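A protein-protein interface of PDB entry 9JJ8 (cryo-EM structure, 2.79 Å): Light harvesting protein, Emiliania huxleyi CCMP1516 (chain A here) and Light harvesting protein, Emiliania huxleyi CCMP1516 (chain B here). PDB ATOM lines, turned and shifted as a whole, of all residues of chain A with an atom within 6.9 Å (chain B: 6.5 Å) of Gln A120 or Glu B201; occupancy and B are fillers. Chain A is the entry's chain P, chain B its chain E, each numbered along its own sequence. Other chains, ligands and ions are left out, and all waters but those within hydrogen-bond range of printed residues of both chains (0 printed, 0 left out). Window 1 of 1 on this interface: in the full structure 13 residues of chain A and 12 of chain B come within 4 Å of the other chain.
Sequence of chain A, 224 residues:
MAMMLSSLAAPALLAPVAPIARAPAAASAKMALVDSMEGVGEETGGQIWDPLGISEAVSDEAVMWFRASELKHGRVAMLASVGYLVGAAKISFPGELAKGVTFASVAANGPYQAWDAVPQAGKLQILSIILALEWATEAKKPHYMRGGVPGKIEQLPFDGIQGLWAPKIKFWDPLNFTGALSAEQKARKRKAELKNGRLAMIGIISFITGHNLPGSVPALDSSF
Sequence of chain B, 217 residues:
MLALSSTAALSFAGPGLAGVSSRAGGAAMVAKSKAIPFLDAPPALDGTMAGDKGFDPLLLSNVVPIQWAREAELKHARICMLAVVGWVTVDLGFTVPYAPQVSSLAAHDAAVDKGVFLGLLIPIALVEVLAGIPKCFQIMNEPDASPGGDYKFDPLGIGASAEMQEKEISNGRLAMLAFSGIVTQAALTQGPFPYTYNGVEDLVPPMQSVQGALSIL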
ATOM      1  N   TRP A 115       8.196  24.365  20.134  1.00  0.00           N
ATOM      2  CA  TRP A 115       8.258  25.194  21.335  1.00  0.00           C
ATOM      3  C   TRP A 115       9.641  25.142  21.970  1.00  0.00           C
ATOM      4  O   TRP A 115      10.099  26.124  22.565  1.00  0.00           O
ATOM      5  CB  TRP A 115       7.187  24.749  22.332  1.00  0.00           C
ATOM      6  CG  TRP A 115       7.201  25.498  23.635  1.00  0.00           C
ATOM      7  CD1 TRP A 115       7.655  25.040  24.836  1.00  0.00           C
ATOM      8  CD2 TRP A 115       6.727  26.830  23.868  1.00  0.00           C
ATOM      9  NE1 TRP A 115       7.499  26.004  25.801  1.00  0.00           N
ATOM     10  CE2 TRP A 115       6.929  27.112  25.232  1.00  0.00           C
ATOM     11  CE3 TRP A 115       6.151  27.812  23.055  1.00  0.00           C
ATOM     12  CZ2 TRP A 115       6.580  28.334  25.803  1.00  0.00           C
ATOM     13  CZ3 TRP A 115       5.805  29.025  23.624  1.00  0.00           C
ATOM     14  CH2 TRP A 115       6.021  29.275  24.984  1.00  0.00           C
ATOM     15  N   ASP A 116      10.323  24.002  21.849  1.00  0.00           N
ATOM     16  CA  ASP A 116      11.670  23.870  22.391  1.00  0.00           C
ATOM     17  C   ASP A 116      12.703  24.643  21.582  1.00  0.00           C
ATOM     18  O   ASP A 116      13.741  25.025  22.131  1.00  0.00           O
ATOM     19  CB  ASP A 116      12.054  22.394  22.457  1.00  0.00           C
ATOM     20  CG  ASP A 116      10.998  21.554  23.141  1.00  0.00           C
ATOM     21  OD1 ASP A 116      10.880  21.642  24.381  1.00  0.00           O
ATOM     22  OD2 ASP A 116      10.271  20.825  22.436  1.00  0.00           O
ATOM     23  N   ALA A 117      12.445  24.882  20.296  1.00  0.00           N
ATOM     24  CA  ALA A 117      13.371  25.638  19.462  1.00  0.00           C
ATOM     25  C   ALA A 117      13.236  27.144  19.642  1.00  0.00           C
ATOM     26  O   ALA A 117      14.071  27.890  19.119  1.00  0.00           O
ATOM     27  CB  ALA A 117      13.170  25.274  17.989  1.00  0.00           C
ATOM     28  N   VAL A 118      12.211  27.600  20.351  1.00  0.00           N
ATOM     29  CA  VAL A 118      12.067  29.023  20.684  1.00  0.00           C
ATOM     30  C   VAL A 118      13.189  29.426  21.631  1.00  0.00           C
ATOM     31  O   VAL A 118      13.586  28.614  22.488  1.00  0.00           O
ATOM     32  CB  VAL A 118      10.690  29.277  21.311  1.00  0.00           C
ATOM     33  CG1 VAL A 118      10.427  30.763  21.514  1.00  0.00           C
ATOM     34  CG2 VAL A 118       9.599  28.668  20.449  1.00  0.00           C
ATOM     35  N   PRO A 119      13.760  30.626  21.500  1.00  0.00           N
ATOM     36  CA  PRO A 119      14.728  31.093  22.500  1.00  0.00           C
ATOM     37  C   PRO A 119      14.095  31.221  23.879  1.00  0.00           C
ATOM     38  O   PRO A 119      12.886  31.426  24.015  1.00  0.00           O
ATOM     39  CB  PRO A 119      15.168  32.457  21.957  1.00  0.00           C
ATOM     40  CG  PRO A 119      14.964  32.350  20.489  1.00  0.00           C
ATOM     41  CD  PRO A 119      13.751  31.485  20.302  1.00  0.00           C
ATOM     42  N   GLN A 120      14.938  31.075  24.907  1.00  0.00           N
ATOM     43  CA  GLN A 120      14.454  30.995  26.284  1.00  0.00           C
ATOM     44  C   GLN A 120      13.795  32.296  26.727  1.00  0.00           C
ATOM     45  O   GLN A 120      12.814  32.275  27.482  1.00  0.00           O
ATOM     46  CB  GLN A 120      15.608  30.643  27.223  1.00  0.00           C
ATOM     47  CG  GLN A 120      16.409  29.412  26.822  1.00  0.00           C
ATOM     48  CD  GLN A 120      15.617  28.126  26.940  1.00  0.00           C
ATOM     49  OE1 GLN A 120      15.012  27.666  25.973  1.00  0.00           O
ATOM     50  NE2 GLN A 120      15.615  27.539  28.131  1.00  0.00           N
ATOM     51  N   ALA A 121      14.324  33.436  26.272  1.00  0.00           N
ATOM     52  CA  ALA A 121      13.762  34.728  26.655  1.00  0.00           C
ATOM     53  C   ALA A 121      12.351  34.908  26.108  1.00  0.00           C
ATOM     54  O   ALA A 121      11.484  35.469  26.787  1.00  0.00           O
ATOM     55  CB  ALA A 121      14.671  35.858  26.175  1.00  0.00           C
ATOM     56  N   GLY A 122      12.101  34.437  24.886  1.00  0.00           N
ATOM     57  CA  GLY A 122      10.768  34.555  24.315  1.00  0.00           C
ATOM     58  C   GLY A 122       9.734  33.722  25.050  1.00  0.00           C
ATOM     59  O   GLY A 122       8.614  34.184  25.299  1.00  0.00           O
ATOM     60  N   LYS A 123      10.097  32.487  25.409  1.00  0.00           N
ATOM     61  CA  LYS A 123       9.218  31.654  26.222  1.00  0.00           C
ATOM     62  C   LYS A 123       8.992  32.275  27.594  1.00  0.00           C
ATOM     63  O   LYS A 123       7.877  32.223  28.132  1.00  0.00           O
ATOM     64  CB  LYS A 123       9.812  30.251  26.349  1.00  0.00           C
ATOM     65  CG  LYS A 123       9.891  29.508  25.025  1.00  0.00           C
ATOM     66  CD  LYS A 123      10.304  28.057  25.200  1.00  0.00           C
ATOM     67  CE  LYS A 123      11.788  27.932  25.482  1.00  0.00           C
ATOM     68  NZ  LYS A 123      12.237  26.511  25.494  1.00  0.00           N
ATOM     69  N   LEU A 124      10.038  32.894  28.158  1.00  0.00           N
ATOM     70  CA  LEU A 124       9.908  33.603  29.427  1.00  0.00           C
ATOM     71  C   LEU A 124       8.897  34.735  29.329  1.00  0.00           C
ATOM     72  O   LEU A 124       8.044  34.895  30.207  1.00  0.00           O
ATOM     73  CB  LEU A 124      11.266  34.154  29.863  1.00  0.00           C
ATOM     74  CG  LEU A 124      11.271  35.006  31.134  1.00  0.00           C
ATOM     75  CD1 LEU A 124      10.804  34.196  32.332  1.00  0.00           C
ATOM     76  CD2 LEU A 124      12.650  35.596  31.384  1.00  0.00           C
ATOM     77  N   GLN A 125       8.968  35.523  28.254  1.00  0.00           N
ATOM     78  CA  GLN A 125       8.064  36.661  28.110  1.00  0.00           C
ATOM     79  C   GLN A 125       6.630  36.203  27.868  1.00  0.00           C
ATOM     80  O   GLN A 125       5.684  36.781  28.421  1.00  0.00           O
ATOM     81  CB  GLN A 125       8.542  37.579  26.986  1.00  0.00           C
ATOM     82  CG  GLN A 125       9.895  38.215  27.260  1.00  0.00           C
ATOM     83  CD  GLN A 125      10.360  39.115  26.138  1.00  0.00           C
ATOM     84  OE1 GLN A 125       9.750  40.148  25.869  1.00  0.00           O
ATOM     85  NE2 GLN A 125      11.435  38.722  25.466  1.00  0.00           N
ATOM     86  N   THR B 196      19.011  29.371  41.662  1.00  0.00           N
ATOM     87  CA  THR B 196      18.583  27.996  41.476  1.00  0.00           C
ATOM     88  C   THR B 196      19.714  27.228  40.809  1.00  0.00           C
ATOM     89  O   THR B 196      20.709  27.807  40.362  1.00  0.00           O
ATOM     90  CB  THR B 196      17.301  27.907  40.638  1.00  0.00           C
ATOM     91  OG1 THR B 196      17.615  28.146  39.262  1.00  0.00           O
ATOM     92  CG2 THR B 196      16.280  28.931  41.104  1.00  0.00           C
ATOM     93  N   ASN B 198      19.653  25.588  37.997  1.00  0.00           N
ATOM     94  CA  ASN B 198      19.664  25.721  36.545  1.00  0.00           C
ATOM     95  C   ASN B 198      19.103  27.062  36.085  1.00  0.00           C
ATOM     96  O   ASN B 198      18.528  27.133  34.999  1.00  0.00           O
ATOM     97  CB  ASN B 198      18.877  24.585  35.885  1.00  0.00           C
ATOM     98  CG  ASN B 198      19.394  23.212  36.264  1.00  0.00           C
ATOM     99  OD1 ASN B 198      20.600  22.995  36.365  1.00  0.00           O
ATOM    100  ND2 ASN B 198      18.478  22.272  36.472  1.00  0.00           N
ATOM    101  N   GLY B 199      19.239  28.120  36.884  1.00  0.00           N
ATOM    102  CA  GLY B 199      18.764  29.424  36.449  1.00  0.00           C
ATOM    103  C   GLY B 199      17.251  29.562  36.530  1.00  0.00           C
ATOM    104  O   GLY B 199      16.576  28.887  37.312  1.00  0.00           O
ATOM    105  N   VAL B 200      16.710  30.459  35.700  1.00  0.00           N
ATOM    106  CA  VAL B 200      15.268  30.699  35.670  1.00  0.00           C
ATOM    107  C   VAL B 200      14.490  29.555  35.044  1.00  0.00           C
ATOM    108  O   VAL B 200      13.258  29.530  35.145  1.00  0.00           O
ATOM    109  CB  VAL B 200      14.935  31.998  34.909  1.00  0.00           C
ATOM    110  CG1 VAL B 200      15.367  33.212  35.710  1.00  0.00           C
ATOM    111  CG2 VAL B 200      15.589  31.995  33.538  1.00  0.00           C
ATOM    112  N   GLU B 201      15.176  28.622  34.380  1.00  0.00           N
ATOM    113  CA  GLU B 201      14.516  27.430  33.859  1.00  0.00           C
ATOM    114  C   GLU B 201      13.938  26.552  34.966  1.00  0.00           C
ATOM    115  O   GLU B 201      12.935  25.868  34.743  1.00  0.00           O
ATOM    116  CB  GLU B 201      15.490  26.644  32.976  1.00  0.00           C
ATOM    117  CG  GLU B 201      15.876  27.342  31.659  1.00  0.00           C
ATOM    118  CD  GLU B 201      16.982  28.385  31.768  1.00  0.00           C
ATOM    119  OE1 GLU B 201      17.543  28.577  32.861  1.00  0.00           O
ATOM    120  OE2 GLU B 201      17.299  29.010  30.734  1.00  0.00           O
ATOM    121  N   ASP B 202      14.539  26.555  36.161  1.00  0.00           N
ATOM    122  CA  ASP B 202      13.901  25.870  37.284  1.00  0.00           C
ATOM    123  C   ASP B 202      12.632  26.576  37.733  1.00  0.00           C
ATOM    124  O   ASP B 202      11.687  25.916  38.180  1.00  0.00           O
ATOM    125  CB  ASP B 202      14.856  25.743  38.471  1.00  0.00           C
ATOM    126  CG  ASP B 202      16.065  24.895  38.162  1.00  0.00           C
ATOM    127  OD1 ASP B 202      15.907  23.839  37.514  1.00  0.00           O
ATOM    128  OD2 ASP B 202      17.171  25.270  38.597  1.00  0.00           O
ATOM    129  N   LEU B 203      12.598  27.908  37.641  1.00  0.00           N
ATOM    130  CA  LEU B 203      11.377  28.639  37.951  1.00  0.00           C
ATOM    131  C   LEU B 203      10.271  28.338  36.951  1.00  0.00           C
ATOM    132  O   LEU B 203       9.105  28.243  37.338  1.00  0.00           O
ATOM    133  CB  LEU B 203      11.651  30.142  37.997  1.00  0.00           C
ATOM    134  CG  LEU B 203      12.689  30.625  39.010  1.00  0.00           C
ATOM    135  CD1 LEU B 203      12.943  32.114  38.850  1.00  0.00           C
ATOM    136  CD2 LEU B 203      12.215  30.317  40.415  1.00  0.00           C
ATOM    137  N   VAL B 204      10.607  28.181  35.674  1.00  0.00           N
ATOM    138  CA  VAL B 204       9.600  27.966  34.637  1.00  0.00           C
ATOM    139  C   VAL B 204       9.781  26.582  34.020  1.00  0.00           C
ATOM    140  O   VAL B 204      10.614  26.414  33.118  1.00  0.00           O
ATOM    141  CB  VAL B 204       9.671  29.059  33.559  1.00  0.00           C
ATOM    142  CG1 VAL B 204       8.437  29.010  32.690  1.00  0.00           C
ATOM    143  CG2 VAL B 204       9.822  30.434  34.194  1.00  0.00           C
ATOM    144  N   PRO B 205       9.041  25.574  34.479  1.00  0.00           N
ATOM    145  CA  PRO B 205       9.155  24.213  33.905  1.00  0.00           C
ATOM    146  C   PRO B 205       8.794  24.107  32.426  1.00  0.00           C
ATOM    147  O   PRO B 205       9.316  23.198  31.763  1.00  0.00           O
ATOM    148  CB  PRO B 205       8.203  23.373  34.778  1.00  0.00           C
ATOM    149  CG  PRO B 205       7.473  24.336  35.661  1.00  0.00           C
ATOM    150  CD  PRO B 205       8.300  25.570  35.751  1.00  0.00           C
ATOM    151  N   PRO B 206       7.911  24.949  31.847  1.00  0.00           N
ATOM    152  CA  PRO B 206       7.756  24.889  30.378  1.00  0.00           C
ATOM    153  C   PRO B 206       9.002  25.249  29.579  1.00  0.00           C
ATOM    154  O   PRO B 206       9.055  24.929  28.385  1.00  0.00           O
ATOM    155  CB  PRO B 206       6.617  25.877  30.108  1.00  0.00           C
ATOM    156  CG  PRO B 206       5.774  25.736  31.270  1.00  0.00           C
ATOM    157  CD  PRO B 206       6.736  25.649  32.417  1.00  0.00           C
ATOM    158  N   MET B 207       9.998  25.904  30.180  1.00  0.00           N
ATOM    159  CA  MET B 207      11.253  26.147  29.477  1.00  0.00           C
ATOM    160  C   MET B 207      12.045  24.870  29.229  1.00  0.00           C
ATOM    161  O   MET B 207      12.898  24.850  28.335  1.00  0.00           O
ATOM    162  CB  MET B 207      12.136  27.111  30.265  1.00  0.00           C
ATOM    163  CG  MET B 207      11.789  28.577  30.145  1.00  0.00           C
ATOM    164  SD  MET B 207      13.259  29.559  30.485  1.00  0.00           S
ATOM    165  CE  MET B 207      12.533  31.035  31.172  1.00  0.00           C
ATOM    166  N   GLN B 208      11.794  23.813  29.996  1.00  0.00           N
ATOM    167  CA  GLN B 208      12.658  22.637  30.037  1.00  0.00           C
ATOM    168  C   GLN B 208      11.958  21.443  29.390  1.00  0.00           C
ATOM    169  O   GLN B 208      11.254  20.691  30.066  1.00  0.00           O
ATOM    170  CB  GLN B 208      13.046  22.308  31.477  1.00  0.00           C
ATOM    171  CG  GLN B 208      13.794  23.402  32.207  1.00  0.00           C
ATOM    172  CD  GLN B 208      13.890  23.130  33.696  1.00  0.00           C
ATOM    173  OE1 GLN B 208      12.878  22.915  34.364  1.00  0.00           O
ATOM    174  NE2 GLN B 208      15.107  23.141  34.224  1.00  0.00           N
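The side-chain carboxylate of Glu B201 sits at hydrogen-bond distance from the side-chain amide nitrogen of Gln A120. The side-chain amino group (NZ) of Lys A123 sits at hydrogen-bond distance from the backbone carbonyl oxygen (O) of Met B207, 3.4 Å away. The backbone carbonyl oxygen (O) of Pro B206 sits at hydrogen-bond distance from the indole nitrogen (NE1) of Trp A115 (3.2 Å).
Hydrophobic or aromatic side chains of chain B within 4 Å of the printed part of chain A: Met B207. Of the 11 printed residues of chain A, 4 touch a printed residue of chain B. Among the printed residues, 5 pairs touch across the chains. Among the printed residues, no Asp or Glu carboxylate lies within 4 Å of a Lys or Arg side-chain nitrogen of the other chain.
The backbone carbonyl oxygen (O) of Glu B201 lies close to the side-chain amide oxygen (OE1) of Gln B208 (3.0 Å). The side-chain amide oxygen (OE1) of Gln A120 is in hydrogen-bond range of the side-chain amino group (NZ) of Lys A123 (3.0 Å).
Gln A120 touches Met B207 (NE2 to O, 3.8 Å). Leu A124 touches Met B207.
Val A118 touches none of the printed residues of chain B. Of chain B, only Glu B201 (3.4 Å) and Met B207 (3.8 Å) come within 4 Å of Gln A120. Printed residues of chain B within 4 Å of Leu A124: Met B207. Glu B201 touches just one residue of chain A: Gln A120 (3.4 Å). Of the printed residues of chain A, Met B207 touches Gln A120 (3.8 Å), Lys A123 (3.4 Å) and Leu A124 (3.6 Å). The nearest printed residue of chain A that does not touch Glu B201 is Ala A121 (7.0 Å).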
